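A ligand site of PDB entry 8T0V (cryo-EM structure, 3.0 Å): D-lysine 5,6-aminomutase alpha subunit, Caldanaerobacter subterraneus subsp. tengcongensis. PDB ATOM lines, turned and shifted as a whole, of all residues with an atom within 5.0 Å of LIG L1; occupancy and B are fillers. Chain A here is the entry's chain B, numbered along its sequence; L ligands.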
ATOM      1  N   ILE A 184      -8.388  -7.524 -24.470  1.00  0.00           N
ATOM      2  CA  ILE A 184      -7.136  -8.276 -24.513  1.00  0.00           C
ATOM      3  C   ILE A 184      -5.982  -7.348 -24.161  1.00  0.00           C
ATOM      4  O   ILE A 184      -5.954  -6.183 -24.559  1.00  0.00           O
ATOM      5  CB  ILE A 184      -6.945  -8.917 -25.890  1.00  0.00           C
ATOM      6  CG1 ILE A 184      -5.823  -9.964 -25.846  1.00  0.00           C
ATOM      7  CG2 ILE A 184      -6.611  -7.874 -26.929  1.00  0.00           C
ATOM      8  CD1 ILE A 184      -6.223 -11.264 -25.190  1.00  0.00           C
ATOM      9  N   ARG A 185      -5.040  -7.868 -23.390  1.00  0.00           N
ATOM     10  CA  ARG A 185      -4.005  -7.047 -22.789  1.00  0.00           C
ATOM     11  C   ARG A 185      -2.885  -6.770 -23.781  1.00  0.00           C
ATOM     12  O   ARG A 185      -2.676  -7.503 -24.745  1.00  0.00           O
ATOM     13  CB  ARG A 185      -3.441  -7.751 -21.555  1.00  0.00           C
ATOM     14  CG  ARG A 185      -2.987  -6.828 -20.462  1.00  0.00           C
ATOM     15  CD  ARG A 185      -2.929  -7.539 -19.136  1.00  0.00           C
ATOM     16  NE  ARG A 185      -2.153  -8.764 -19.234  1.00  0.00           N
ATOM     17  CZ  ARG A 185      -1.521  -9.344 -18.214  1.00  0.00           C
ATOM     18  NH1 ARG A 185      -1.541  -8.816 -17.008  1.00  0.00           N
ATOM     19  NH2 ARG A 185      -0.848 -10.469 -18.425  1.00  0.00           N
ATOM     20  N   ALA A 186      -2.158  -5.684 -23.522  1.00  0.00           N
ATOM     21  CA  ALA A 186      -1.072  -5.292 -24.410  1.00  0.00           C
ATOM     22  C   ALA A 186       0.032  -6.334 -24.393  1.00  0.00           C
ATOM     23  O   ALA A 186       0.363  -6.892 -23.346  1.00  0.00           O
ATOM     24  CB  ALA A 186      -0.510  -3.931 -24.004  1.00  0.00           C
ATOM     25  N   SER A 190       2.839  -8.932 -19.382  1.00  0.00           N
ATOM     26  CA  SER A 190       3.132 -10.010 -18.462  1.00  0.00           C
ATOM     27  C   SER A 190       4.592  -9.980 -18.012  1.00  0.00           C
ATOM     28  O   SER A 190       4.900 -10.488 -16.926  1.00  0.00           O
ATOM     29  CB  SER A 190       2.825 -11.355 -19.110  1.00  0.00           C
ATOM     30  OG  SER A 190       3.567 -12.395 -18.498  1.00  0.00           O
ATOM     31  N   TYR A 237      -7.379 -10.056 -17.672  1.00  0.00           N
ATOM     32  CA  TYR A 237      -6.427 -11.144 -17.508  1.00  0.00           C
ATOM     33  C   TYR A 237      -5.523 -10.829 -16.335  1.00  0.00           C
ATOM     34  O   TYR A 237      -4.922  -9.758 -16.263  1.00  0.00           O
ATOM     35  CB  TYR A 237      -5.614 -11.338 -18.790  1.00  0.00           C
ATOM     36  CG  TYR A 237      -6.476 -11.469 -20.020  1.00  0.00           C
ATOM     37  CD1 TYR A 237      -7.086 -10.375 -20.596  1.00  0.00           C
ATOM     38  CD2 TYR A 237      -6.698 -12.716 -20.585  1.00  0.00           C
ATOM     39  CE1 TYR A 237      -7.894 -10.506 -21.698  1.00  0.00           C
ATOM     40  CE2 TYR A 237      -7.500 -12.856 -21.689  1.00  0.00           C
ATOM     41  CZ  TYR A 237      -8.086 -11.748 -22.249  1.00  0.00           C
ATOM     42  OH  TYR A 237      -8.894 -11.889 -23.360  1.00  0.00           O
ATOM     43  N   SER A 239      -2.751 -12.549 -15.527  1.00  0.00           N
ATOM     44  CA  SER A 239      -1.481 -13.229 -15.714  1.00  0.00           C
ATOM     45  C   SER A 239      -0.321 -12.248 -15.582  1.00  0.00           C
ATOM     46  O   SER A 239      -0.503 -11.039 -15.519  1.00  0.00           O
ATOM     47  CB  SER A 239      -1.444 -13.914 -17.075  1.00  0.00           C
ATOM     48  OG  SER A 239      -2.476 -14.879 -17.193  1.00  0.00           O
ATOM     49  N   GLY A 240       0.882 -12.791 -15.531  1.00  0.00           N
ATOM     50  CA  GLY A 240       2.100 -12.002 -15.533  1.00  0.00           C
ATOM     51  C   GLY A 240       2.860 -12.093 -14.223  1.00  0.00           C
ATOM     52  O   GLY A 240       2.622 -12.969 -13.384  1.00  0.00           O
ATOM     53  N   LEU A 259      -9.244 -13.988 -16.191  1.00  0.00           N
ATOM     54  CA  LEU A 259      -8.501 -15.151 -16.679  1.00  0.00           C
ATOM     55  C   LEU A 259      -7.335 -15.424 -15.748  1.00  0.00           C
ATOM     56  O   LEU A 259      -6.307 -14.740 -15.803  1.00  0.00           O
ATOM     57  CB  LEU A 259      -8.024 -14.918 -18.103  1.00  0.00           C
ATOM     58  CG  LEU A 259      -8.986 -15.395 -19.199  1.00  0.00           C
ATOM     59  CD1 LEU A 259      -9.983 -14.312 -19.550  1.00  0.00           C
ATOM     60  CD2 LEU A 259      -8.206 -15.832 -20.420  1.00  0.00           C
ATOM     61  N   ASP A 261      -4.899 -18.328 -14.638  1.00  0.00           N
ATOM     62  CA  ASP A 261      -4.243 -19.625 -14.761  1.00  0.00           C
ATOM     63  C   ASP A 261      -2.734 -19.401 -14.721  1.00  0.00           C
ATOM     64  O   ASP A 261      -2.215 -18.495 -15.380  1.00  0.00           O
ATOM     65  CB  ASP A 261      -4.631 -20.351 -16.053  1.00  0.00           C
ATOM     66  CG  ASP A 261      -4.440 -21.853 -15.967  1.00  0.00           C
ATOM     67  OD1 ASP A 261      -4.057 -22.343 -14.879  1.00  0.00           O
ATOM     68  OD2 ASP A 261      -4.644 -22.541 -16.983  1.00  0.00           O
ATOM     69  N   TYR A 264      -0.608 -21.384 -17.969  1.00  0.00           N
ATOM     70  CA  TYR A 264      -0.400 -20.577 -19.168  1.00  0.00           C
ATOM     71  C   TYR A 264       0.844 -19.714 -19.019  1.00  0.00           C
ATOM     72  O   TYR A 264       1.677 -19.661 -19.919  1.00  0.00           O
ATOM     73  CB  TYR A 264      -1.599 -19.684 -19.465  1.00  0.00           C
ATOM     74  CG  TYR A 264      -1.306 -18.715 -20.590  1.00  0.00           C
ATOM     75  CD1 TYR A 264      -1.583 -19.046 -21.913  1.00  0.00           C
ATOM     76  CD2 TYR A 264      -0.698 -17.488 -20.342  1.00  0.00           C
ATOM     77  CE1 TYR A 264      -1.302 -18.173 -22.941  1.00  0.00           C
ATOM     78  CE2 TYR A 264      -0.406 -16.617 -21.378  1.00  0.00           C
ATOM     79  CZ  TYR A 264      -0.717 -16.968 -22.669  1.00  0.00           C
ATOM     80  OH  TYR A 264      -0.430 -16.102 -23.698  1.00  0.00           O
ATOM     81  N   ARG A 269       4.616 -17.851 -21.486  1.00  0.00           N
ATOM     82  CA  ARG A 269       5.350 -16.616 -21.247  1.00  0.00           C
ATOM     83  C   ARG A 269       6.710 -16.868 -20.606  1.00  0.00           C
ATOM     84  O   ARG A 269       7.501 -15.935 -20.474  1.00  0.00           O
ATOM     85  CB  ARG A 269       4.540 -15.668 -20.368  1.00  0.00           C
ATOM     86  CG  ARG A 269       3.146 -15.351 -20.900  1.00  0.00           C
ATOM     87  CD  ARG A 269       3.164 -14.778 -22.314  1.00  0.00           C
ATOM     88  NE  ARG A 269       4.106 -13.660 -22.444  1.00  0.00           N
ATOM     89  CZ  ARG A 269       3.836 -12.509 -23.040  1.00  0.00           C
ATOM     90  NH1 ARG A 269       2.668 -12.270 -23.602  1.00  0.00           N
ATOM     91  NH2 ARG A 269       4.772 -11.568 -23.076  1.00  0.00           N
ATOM     92  N   THR A 296      -9.802 -20.489 -16.958  1.00  0.00           N
ATOM     93  CA  THR A 296      -8.528 -21.147 -17.235  1.00  0.00           C
ATOM     94  C   THR A 296      -8.311 -21.283 -18.734  1.00  0.00           C
ATOM     95  O   THR A 296      -9.223 -21.088 -19.543  1.00  0.00           O
ATOM     96  CB  THR A 296      -8.476 -22.506 -16.553  1.00  0.00           C
ATOM     97  OG1 THR A 296      -9.280 -23.444 -17.278  1.00  0.00           O
ATOM     98  CG2 THR A 296      -8.989 -22.411 -15.126  1.00  0.00           C
ATOM     99  N   GLY A 297      -7.092 -21.644 -19.101  1.00  0.00           N
ATOM    100  CA  GLY A 297      -6.652 -21.550 -20.487  1.00  0.00           C
ATOM    101  C   GLY A 297      -6.129 -22.819 -21.120  1.00  0.00           C
ATOM    102  O   GLY A 297      -5.076 -22.783 -21.777  1.00  0.00           O
ATOM    103  N   ASP A 299      -7.265 -24.143 -23.618  1.00  0.00           N
ATOM    104  CA  ASP A 299      -7.359 -24.003 -25.067  1.00  0.00           C
ATOM    105  C   ASP A 299      -5.972 -23.877 -25.686  1.00  0.00           C
ATOM    106  O   ASP A 299      -5.745 -24.329 -26.816  1.00  0.00           O
ATOM    107  CB  ASP A 299      -8.181 -22.771 -25.436  1.00  0.00           C
ATOM    108  CG  ASP A 299      -7.887 -21.569 -24.543  1.00  0.00           C
ATOM    109  OD1 ASP A 299      -8.258 -21.593 -23.354  1.00  0.00           O
ATOM    110  OD2 ASP A 299      -7.291 -20.590 -25.038  1.00  0.00           O
ATOM    111  N   ASN A 300      -5.040 -23.249 -24.963  1.00  0.00           N
ATOM    112  CA  ASN A 300      -3.737 -22.941 -25.542  1.00  0.00           C
ATOM    113  C   ASN A 300      -2.888 -24.179 -25.731  1.00  0.00           C
ATOM    114  O   ASN A 300      -1.929 -24.162 -26.504  1.00  0.00           O
ATOM    115  CB  ASN A 300      -3.012 -21.935 -24.649  1.00  0.00           C
ATOM    116  CG  ASN A 300      -3.722 -20.607 -24.562  1.00  0.00           C
ATOM    117  OD1 ASN A 300      -3.773 -19.843 -25.531  1.00  0.00           O
ATOM    118  ND2 ASN A 300      -4.297 -20.320 -23.405  1.00  0.00           N
ATOM    119  N   THR A 303      -2.936 -25.563 -29.469  1.00  0.00           N
ATOM    120  CA  THR A 303      -2.266 -24.822 -30.527  1.00  0.00           C
ATOM    121  C   THR A 303      -0.805 -25.226 -30.686  1.00  0.00           C
ATOM    122  O   THR A 303      -0.189 -24.891 -31.703  1.00  0.00           O
ATOM    123  CB  THR A 303      -2.352 -23.319 -30.262  1.00  0.00           C
ATOM    124  OG1 THR A 303      -1.514 -22.976 -29.154  1.00  0.00           O
ATOM    125  CG2 THR A 303      -3.787 -22.903 -29.958  1.00  0.00           C
ATOM    126  N   THR A 376      -8.668 -22.156 -33.780  1.00  0.00           N
ATOM    127  CA  THR A 376      -7.671 -21.157 -34.159  1.00  0.00           C
ATOM    128  C   THR A 376      -6.543 -21.766 -34.971  1.00  0.00           C
ATOM    129  O   THR A 376      -6.071 -21.157 -35.936  1.00  0.00           O
ATOM    130  CB  THR A 376      -7.097 -20.495 -32.921  1.00  0.00           C
ATOM    131  OG1 THR A 376      -6.294 -19.371 -33.314  1.00  0.00           O
ATOM    132  CG2 THR A 376      -6.226 -21.494 -32.174  1.00  0.00           C
ATOM    133  N   GLU A 412      -9.929 -14.920 -38.372  1.00  0.00           N
ATOM    134  CA  GLU A 412      -8.958 -15.164 -37.315  1.00  0.00           C
ATOM    135  C   GLU A 412      -7.542 -15.236 -37.859  1.00  0.00           C
ATOM    136  O   GLU A 412      -6.618 -14.647 -37.273  1.00  0.00           O
ATOM    137  CB  GLU A 412      -9.288 -16.465 -36.582  1.00  0.00           C
ATOM    138  CG  GLU A 412     -10.458 -16.356 -35.611  1.00  0.00           C
ATOM    139  CD  GLU A 412     -10.601 -17.588 -34.731  1.00  0.00           C
ATOM    140  OE1 GLU A 412      -9.647 -17.901 -33.991  1.00  0.00           O
ATOM    141  OE2 GLU A 412     -11.662 -18.244 -34.793  1.00  0.00           O
HETATM  142  C1  LIG L   1      -5.039 -18.285 -19.722  1.00  0.00           C
HETATM  143  C2  LIG L   1      -4.591 -16.438 -29.688  1.00  0.00           C
HETATM  144  C3  LIG L   1      -5.620 -17.254 -30.519  1.00  0.00           C
HETATM  145  C4  LIG L   1      -6.295 -16.395 -31.683  1.00  0.00           C
HETATM  146  C5  LIG L   1      -4.598 -16.653 -21.553  1.00  0.00           C
HETATM  147  C6  LIG L   1      -4.607 -16.904 -20.181  1.00  0.00           C
HETATM  148  C7  LIG L   1      -3.909 -14.832 -19.714  1.00  0.00           C
HETATM  149  C8  LIG L   1      -3.751 -14.493 -21.035  1.00  0.00           C
HETATM  150  C9  LIG L   1      -3.268 -13.065 -21.248  1.00  0.00           C
HETATM  151  C10 LIG L   1      -4.138 -15.424 -21.979  1.00  0.00           C
HETATM  152  C11 LIG L   1      -4.049 -15.076 -23.289  1.00  0.00           C
HETATM  153  C12 LIG L   1      -4.163 -15.217 -25.647  1.00  0.00           C
HETATM  154  C13 LIG L   1      -4.576 -16.230 -26.766  1.00  0.00           C
HETATM  155  N1  LIG L   1      -4.289 -16.011 -19.301  1.00  0.00           N
HETATM  156  N2  LIG L   1      -4.344 -15.819 -24.306  1.00  0.00           N
HETATM  157  N3  LIG L   1      -4.994 -18.592 -31.011  1.00  0.00           N
HETATM  158  O1  LIG L   1      -1.982 -13.067 -21.861  1.00  0.00           O
HETATM  159  O2  LIG L   1      -0.300 -12.545 -20.025  1.00  0.00           O
HETATM  160  O3  LIG L   1      -1.341 -10.731 -21.064  1.00  0.00           O
HETATM  161  O4  LIG L   1       0.260 -12.007 -22.306  1.00  0.00           O
HETATM  162  O5  LIG L   1      -6.515 -16.957 -32.744  1.00  0.00           O
HETATM  163  O6  LIG L   1      -6.652 -15.248 -31.475  1.00  0.00           O
HETATM  164  O7  LIG L   1      -5.007 -17.574 -22.444  1.00  0.00           O
HETATM  165  P1  LIG L   1      -0.837 -12.099 -21.320  1.00  0.00           P
HETATM  166  S1  LIG L   1      -5.265 -15.389 -28.294  1.00  0.00           S
HETATM  167 CO1  LG2 L   2      -1.514 -15.558 -31.686  1.00  0.00          CO
HETATM  168  N1  LG2 L   2      -2.006 -14.340 -33.042  1.00  0.00           N
HETATM  169  N2  LG2 L   2      -1.368 -14.104 -30.427  1.00  0.00           N
HETATM  170  N3  LG2 L   2      -0.961 -17.078 -30.481  1.00  0.00           N
HETATM  171  N4  LG2 L   2      -2.086 -17.028 -32.887  1.00  0.00           N
HETATM  172  C1  LG2 L   2      -2.389 -14.992 -34.312  1.00  0.00           C
HETATM  173  C2  LG2 L   2      -1.037 -15.078 -35.117  1.00  0.00           C
HETATM  174  C3  LG2 L   2      -3.449 -13.940 -34.906  1.00  0.00           C
HETATM  175  C4  LG2 L   2      -3.485 -13.923 -36.461  1.00  0.00           C
HETATM  176  C5  LG2 L   2      -4.915 -14.211 -34.358  1.00  0.00           C
HETATM  177  C6  LG2 L   2      -5.959 -13.119 -34.454  1.00  0.00           C
HETATM  178  O1  LG2 L   2      -6.430 -12.620 -33.610  1.00  0.00           O
HETATM  179  N5  LG2 L   2      -6.345 -12.695 -35.541  1.00  0.00           N
HETATM  180  C7  LG2 L   2      -2.933 -12.594 -34.249  1.00  0.00           C
HETATM  181  C8  LG2 L   2      -1.974 -11.704 -35.112  1.00  0.00           C
HETATM  182  C9  LG2 L   2      -2.728 -10.819 -36.146  1.00  0.00           C
HETATM  183  C10 LG2 L   2      -2.099  -9.471 -36.365  1.00  0.00           C
HETATM  184  O2  LG2 L   2      -1.493  -9.174 -37.360  1.00  0.00           O
HETATM  185  N6  LG2 L   2      -2.293  -8.570 -35.367  1.00  0.00           N
HETATM  186  C11 LG2 L   2      -2.315 -13.094 -32.946  1.00  0.00           C
HETATM  187  C12 LG2 L   2      -2.168 -12.334 -31.820  1.00  0.00           C
HETATM  188  C13 LG2 L   2      -2.601 -10.851 -31.896  1.00  0.00           C
HETATM  189  C14 LG2 L   2      -1.690 -12.828 -30.620  1.00  0.00           C
HETATM  190  C15 LG2 L   2      -1.362 -12.004 -29.343  1.00  0.00           C
HETATM  191  C16 LG2 L   2      -0.045 -11.202 -29.583  1.00  0.00           C
HETATM  192  C17 LG2 L   2      -2.487 -11.025 -28.809  1.00  0.00           C
HETATM  193  C18 LG2 L   2      -2.237 -10.452 -27.407  1.00  0.00           C
HETATM  194  O3  LG2 L   2      -1.708  -9.386 -27.212  1.00  0.00           O
HETATM  195  N7  LG2 L   2      -2.687 -11.190 -26.361  1.00  0.00           N
HETATM  196  C19 LG2 L   2      -1.191 -13.161 -28.312  1.00  0.00           C
HETATM  197  C20 LG2 L   2      -0.004 -13.042 -27.303  1.00  0.00           C
HETATM  198  C21 LG2 L   2       1.365 -13.559 -27.835  1.00  0.00           C
HETATM  199  C22 LG2 L   2       2.479 -12.531 -27.830  1.00  0.00           C
HETATM  200  O4  LG2 L   2       3.091 -12.204 -28.827  1.00  0.00           O
HETATM  201  N8  LG2 L   2       2.831 -12.043 -26.621  1.00  0.00           N
HETATM  202  C23 LG2 L   2      -1.182 -14.400 -29.164  1.00  0.00           C
HETATM  203  C24 LG2 L   2      -0.872 -15.608 -28.632  1.00  0.00           C
HETATM  204  C25 LG2 L   2      -0.742 -16.814 -29.220  1.00  0.00           C
HETATM  205  C26 LG2 L   2      -0.201 -18.014 -28.461  1.00  0.00           C
HETATM  206  C27 LG2 L   2      -1.240 -18.541 -27.443  1.00  0.00           C
HETATM  207  C28 LG2 L   2       1.101 -17.614 -27.694  1.00  0.00           C
HETATM  208  C29 LG2 L   2      -0.031 -19.034 -29.634  1.00  0.00           C
HETATM  209  C30 LG2 L   2       1.442 -19.409 -29.996  1.00  0.00           C
HETATM  210  C31 LG2 L   2       1.973 -20.596 -29.155  1.00  0.00           C
HETATM  211  C32 LG2 L   2       3.481 -20.701 -29.246  1.00  0.00           C
HETATM  212  O5  LG2 L   2       4.078 -20.563 -30.296  1.00  0.00           O
HETATM  213  N9  LG2 L   2       4.159 -20.907 -28.094  1.00  0.00           N
HETATM  214  C33 LG2 L   2      -0.749 -18.334 -30.800  1.00  0.00           C
HETATM  215  C34 LG2 L   2      -1.098 -18.941 -31.982  1.00  0.00           C
HETATM  216  C35 LG2 L   2      -0.716 -20.417 -32.171  1.00  0.00           C
HETATM  217  C36 LG2 L   2      -1.788 -18.271 -32.975  1.00  0.00           C
HETATM  218  C37 LG2 L   2      -2.376 -18.879 -34.274  1.00  0.00           C
HETATM  219  C38 LG2 L   2      -3.560 -19.768 -33.881  1.00  0.00           C
HETATM  220  C39 LG2 L   2      -1.436 -19.720 -35.200  1.00  0.00           C
HETATM  221  C40 LG2 L   2      -0.128 -18.999 -35.616  1.00  0.00           C
HETATM  222  C41 LG2 L   2       0.912 -19.981 -36.082  1.00  0.00           C
HETATM  223  O6  LG2 L   2       1.989 -20.056 -35.535  1.00  0.00           O
HETATM  224  N10 LG2 L   2       0.548 -20.782 -37.130  1.00  0.00           N
HETATM  225  C42 LG2 L   2      -2.862 -17.582 -35.057  1.00  0.00           C
HETATM  226  C43 LG2 L   2      -4.172 -17.714 -35.915  1.00  0.00           C
HETATM  227  C44 LG2 L   2      -3.968 -18.403 -37.259  1.00  0.00           C
HETATM  228  O7  LG2 L   2      -3.079 -18.120 -38.034  1.00  0.00           O
HETATM  229  N11 LG2 L   2      -4.878 -19.355 -37.594  1.00  0.00           N
HETATM  230  C45 LG2 L   2      -2.920 -16.473 -33.964  1.00  0.00           C
HETATM  231  C46 LG2 L   2       1.216 -22.060 -37.467  1.00  0.00           C
HETATM  232  C47 LG2 L   2       2.564 -21.893 -38.228  1.00  0.00           C
HETATM  233  C48 LG2 L   2       3.182 -23.251 -38.600  1.00  0.00           C
HETATM  234  O8  LG2 L   2       2.370 -21.156 -39.444  1.00  0.00           O
HETATM  235  O9  LG2 L   2       3.341 -18.786 -38.822  1.00  0.00           O
HETATM  236  O10 LG2 L   2       2.702 -19.464 -41.173  1.00  0.00           O
HETATM  237  P1  LG2 L   2       3.298 -19.886 -39.788  1.00  0.00           P
HETATM  238  O11 LG2 L   2       4.718 -20.494 -40.196  1.00  0.00           O
HETATM  239  C49 LG2 L   2       5.085 -20.949 -41.526  1.00  0.00           C
HETATM  240  C50 LG2 L   2       5.505 -19.774 -42.468  1.00  0.00           C
HETATM  241  O12 LG2 L   2       4.957 -18.491 -42.148  1.00  0.00           O
HETATM  242  C51 LG2 L   2       7.047 -19.817 -42.490  1.00  0.00           C
HETATM  243  O13 LG2 L   2       7.295 -21.219 -42.378  1.00  0.00           O
HETATM  244  C52 LG2 L   2       6.389 -21.787 -41.408  1.00  0.00           C
HETATM  245  C53 LG2 L   2       6.184 -23.280 -41.728  1.00  0.00           C
HETATM  246  O14 LG2 L   2       5.581 -23.445 -43.015  1.00  0.00           O
HETATM  247  N12 LG2 L   2       7.754 -19.091 -41.430  1.00  0.00           N
HETATM  248  C54 LG2 L   2       9.057 -18.688 -41.412  1.00  0.00           C
HETATM  249  C55 LG2 L   2       7.349 -18.593 -40.191  1.00  0.00           C
HETATM  250  N13 LG2 L   2       8.246 -17.960 -39.495  1.00  0.00           N
HETATM  251  C56 LG2 L   2       9.299 -18.017 -40.250  1.00  0.00           C
HETATM  252  C57 LG2 L   2      10.552 -17.465 -39.984  1.00  0.00           C
HETATM  253  C58 LG2 L   2      11.561 -17.608 -40.951  1.00  0.00           C
HETATM  254  C59 LG2 L   2      12.916 -16.966 -40.691  1.00  0.00           C
HETATM  255  C60 LG2 L   2      11.313 -18.327 -42.144  1.00  0.00           C
HETATM  256  C61 LG2 L   2      12.409 -18.518 -43.173  1.00  0.00           C
HETATM  257  C62 LG2 L   2      10.038 -18.874 -42.394  1.00  0.00           C
HETATM  258  N1  LG3 L   3      -8.909 -20.355 -29.638  1.00  0.00           N
HETATM  259  C1  LG3 L   3      -8.464 -20.354 -28.380  1.00  0.00           C
HETATM  260  N2  LG3 L   3      -8.383 -19.292 -27.574  1.00  0.00           N
HETATM  261  C2  LG3 L   3      -8.693 -18.122 -28.107  1.00  0.00           C
HETATM  262  N3  LG3 L   3      -8.760 -16.890 -27.536  1.00  0.00           N
HETATM  263  C3  LG3 L   3      -9.041 -16.044 -28.620  1.00  0.00           C
HETATM  264  N4  LG3 L   3      -9.369 -16.713 -29.743  1.00  0.00           N
HETATM  265  C4  LG3 L   3      -9.095 -17.996 -29.391  1.00  0.00           C
HETATM  266  C5  LG3 L   3      -9.212 -19.167 -30.117  1.00  0.00           C
HETATM  267  N5  LG3 L   3      -9.780 -19.263 -31.312  1.00  0.00           N
HETATM  268  C6  LG3 L   3      -9.267 -16.643 -26.195  1.00  0.00           C
HETATM  269  C7  LG3 L   3      -8.354 -16.944 -24.967  1.00  0.00           C
HETATM  270  C8  LG3 L   3      -8.650 -15.731 -24.055  1.00  0.00           C
HETATM  271  C9  LG3 L   3      -8.808 -14.616 -25.080  1.00  0.00           C
HETATM  272  C10 LG3 L   3      -7.481 -14.134 -25.675  1.00  0.00           C
HETATM  273  O1  LG3 L   3      -9.585 -15.240 -26.095  1.00  0.00           O
HETATM  274  O2  LG3 L   3      -8.600 -18.189 -24.319  1.00  0.00           O
HETATM  275  O3  LG3 L   3      -9.921 -15.807 -23.386  1.00  0.00           O
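O5 of LIG L1 sits at hydrogen-bond distance from OG1 of Thr 376, at 2.5 Å.
The guanidinium group (NH2) of Arg 185 lies within salt-bridge range of an oxygen (O2) of LIG L1 (2.7 Å).
NH1 of Arg 269 lies within salt-bridge range of O4 of LIG L1, 2.7 Å away.
A nitrogen (N1) of LIG L1 sits close to the side-chain hydroxyl (OG) of Ser 239 (3.0 Å).
ND2 of Asn 300 lies within hydrogen-bond range of O7 of LIG L1, at 3.0 Å.
A nitrogen (N11) of LG2 L2 sits at hydrogen-bond distance from the backbone carbonyl oxygen of Thr 376 (2.7 Å).
A nitrogen (N5) of LG2 L2 sits at hydrogen-bond distance from the backbone carbonyl oxygen of Glu 412 (2.6 Å).
The side-chain carboxylate (OE1) of Glu 412 sits at hydrogen-bond distance from a nitrogen (N5) of LG3 L3 (3.0 Å).
O2 of LG3 L3 sits at hydrogen-bond distance from OD2 of Asp 299.
NH1 of Arg 185 lies within hydrogen-bond range of O of Ser 239 (2.9 Å).
O of Gly 297 sits at hydrogen-bond distance from ND2 of Asn 300 (3.1 Å).
OD2 of Asp 299 sits at hydrogen-bond distance from ND2 of Asn 300 (3.4 Å).
The backbone carbonyl oxygen (O) of Asn 300 is in hydrogen-bond range of the side-chain hydroxyl (OG1) of Thr 303, 2.9 Å away.
N of Gly 297 is in hydrogen-bond range of OD2 of Asp 261 (3.4 Å).
CB of Ser 190 touches O2 of LIG L1, at 3.5 Å.
CD2 of Tyr 237 touches C8 of LIG L1 (3.5 Å).
CD2 of Leu 259 touches C6 of LIG L1, 3.8 Å away.
Tyr 264 touches LIG L1.
CA of Gly 297 touches C1 of LIG L1 (3.7 Å).
Glu 412 touches LIG L1 (OE1 to O5, 3.5 Å).
Hydrophobic or aromatic side chains within 4 Å of LIG L1: Tyr 237, Leu 259 and Tyr 264.
Within 4 Å of LIG L1: Arg 185, Ser 190, Tyr 237, Ser 239, Leu 259, Tyr 264, Arg 269, Gly 297, Asn 300, Thr 376 and Glu 412.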
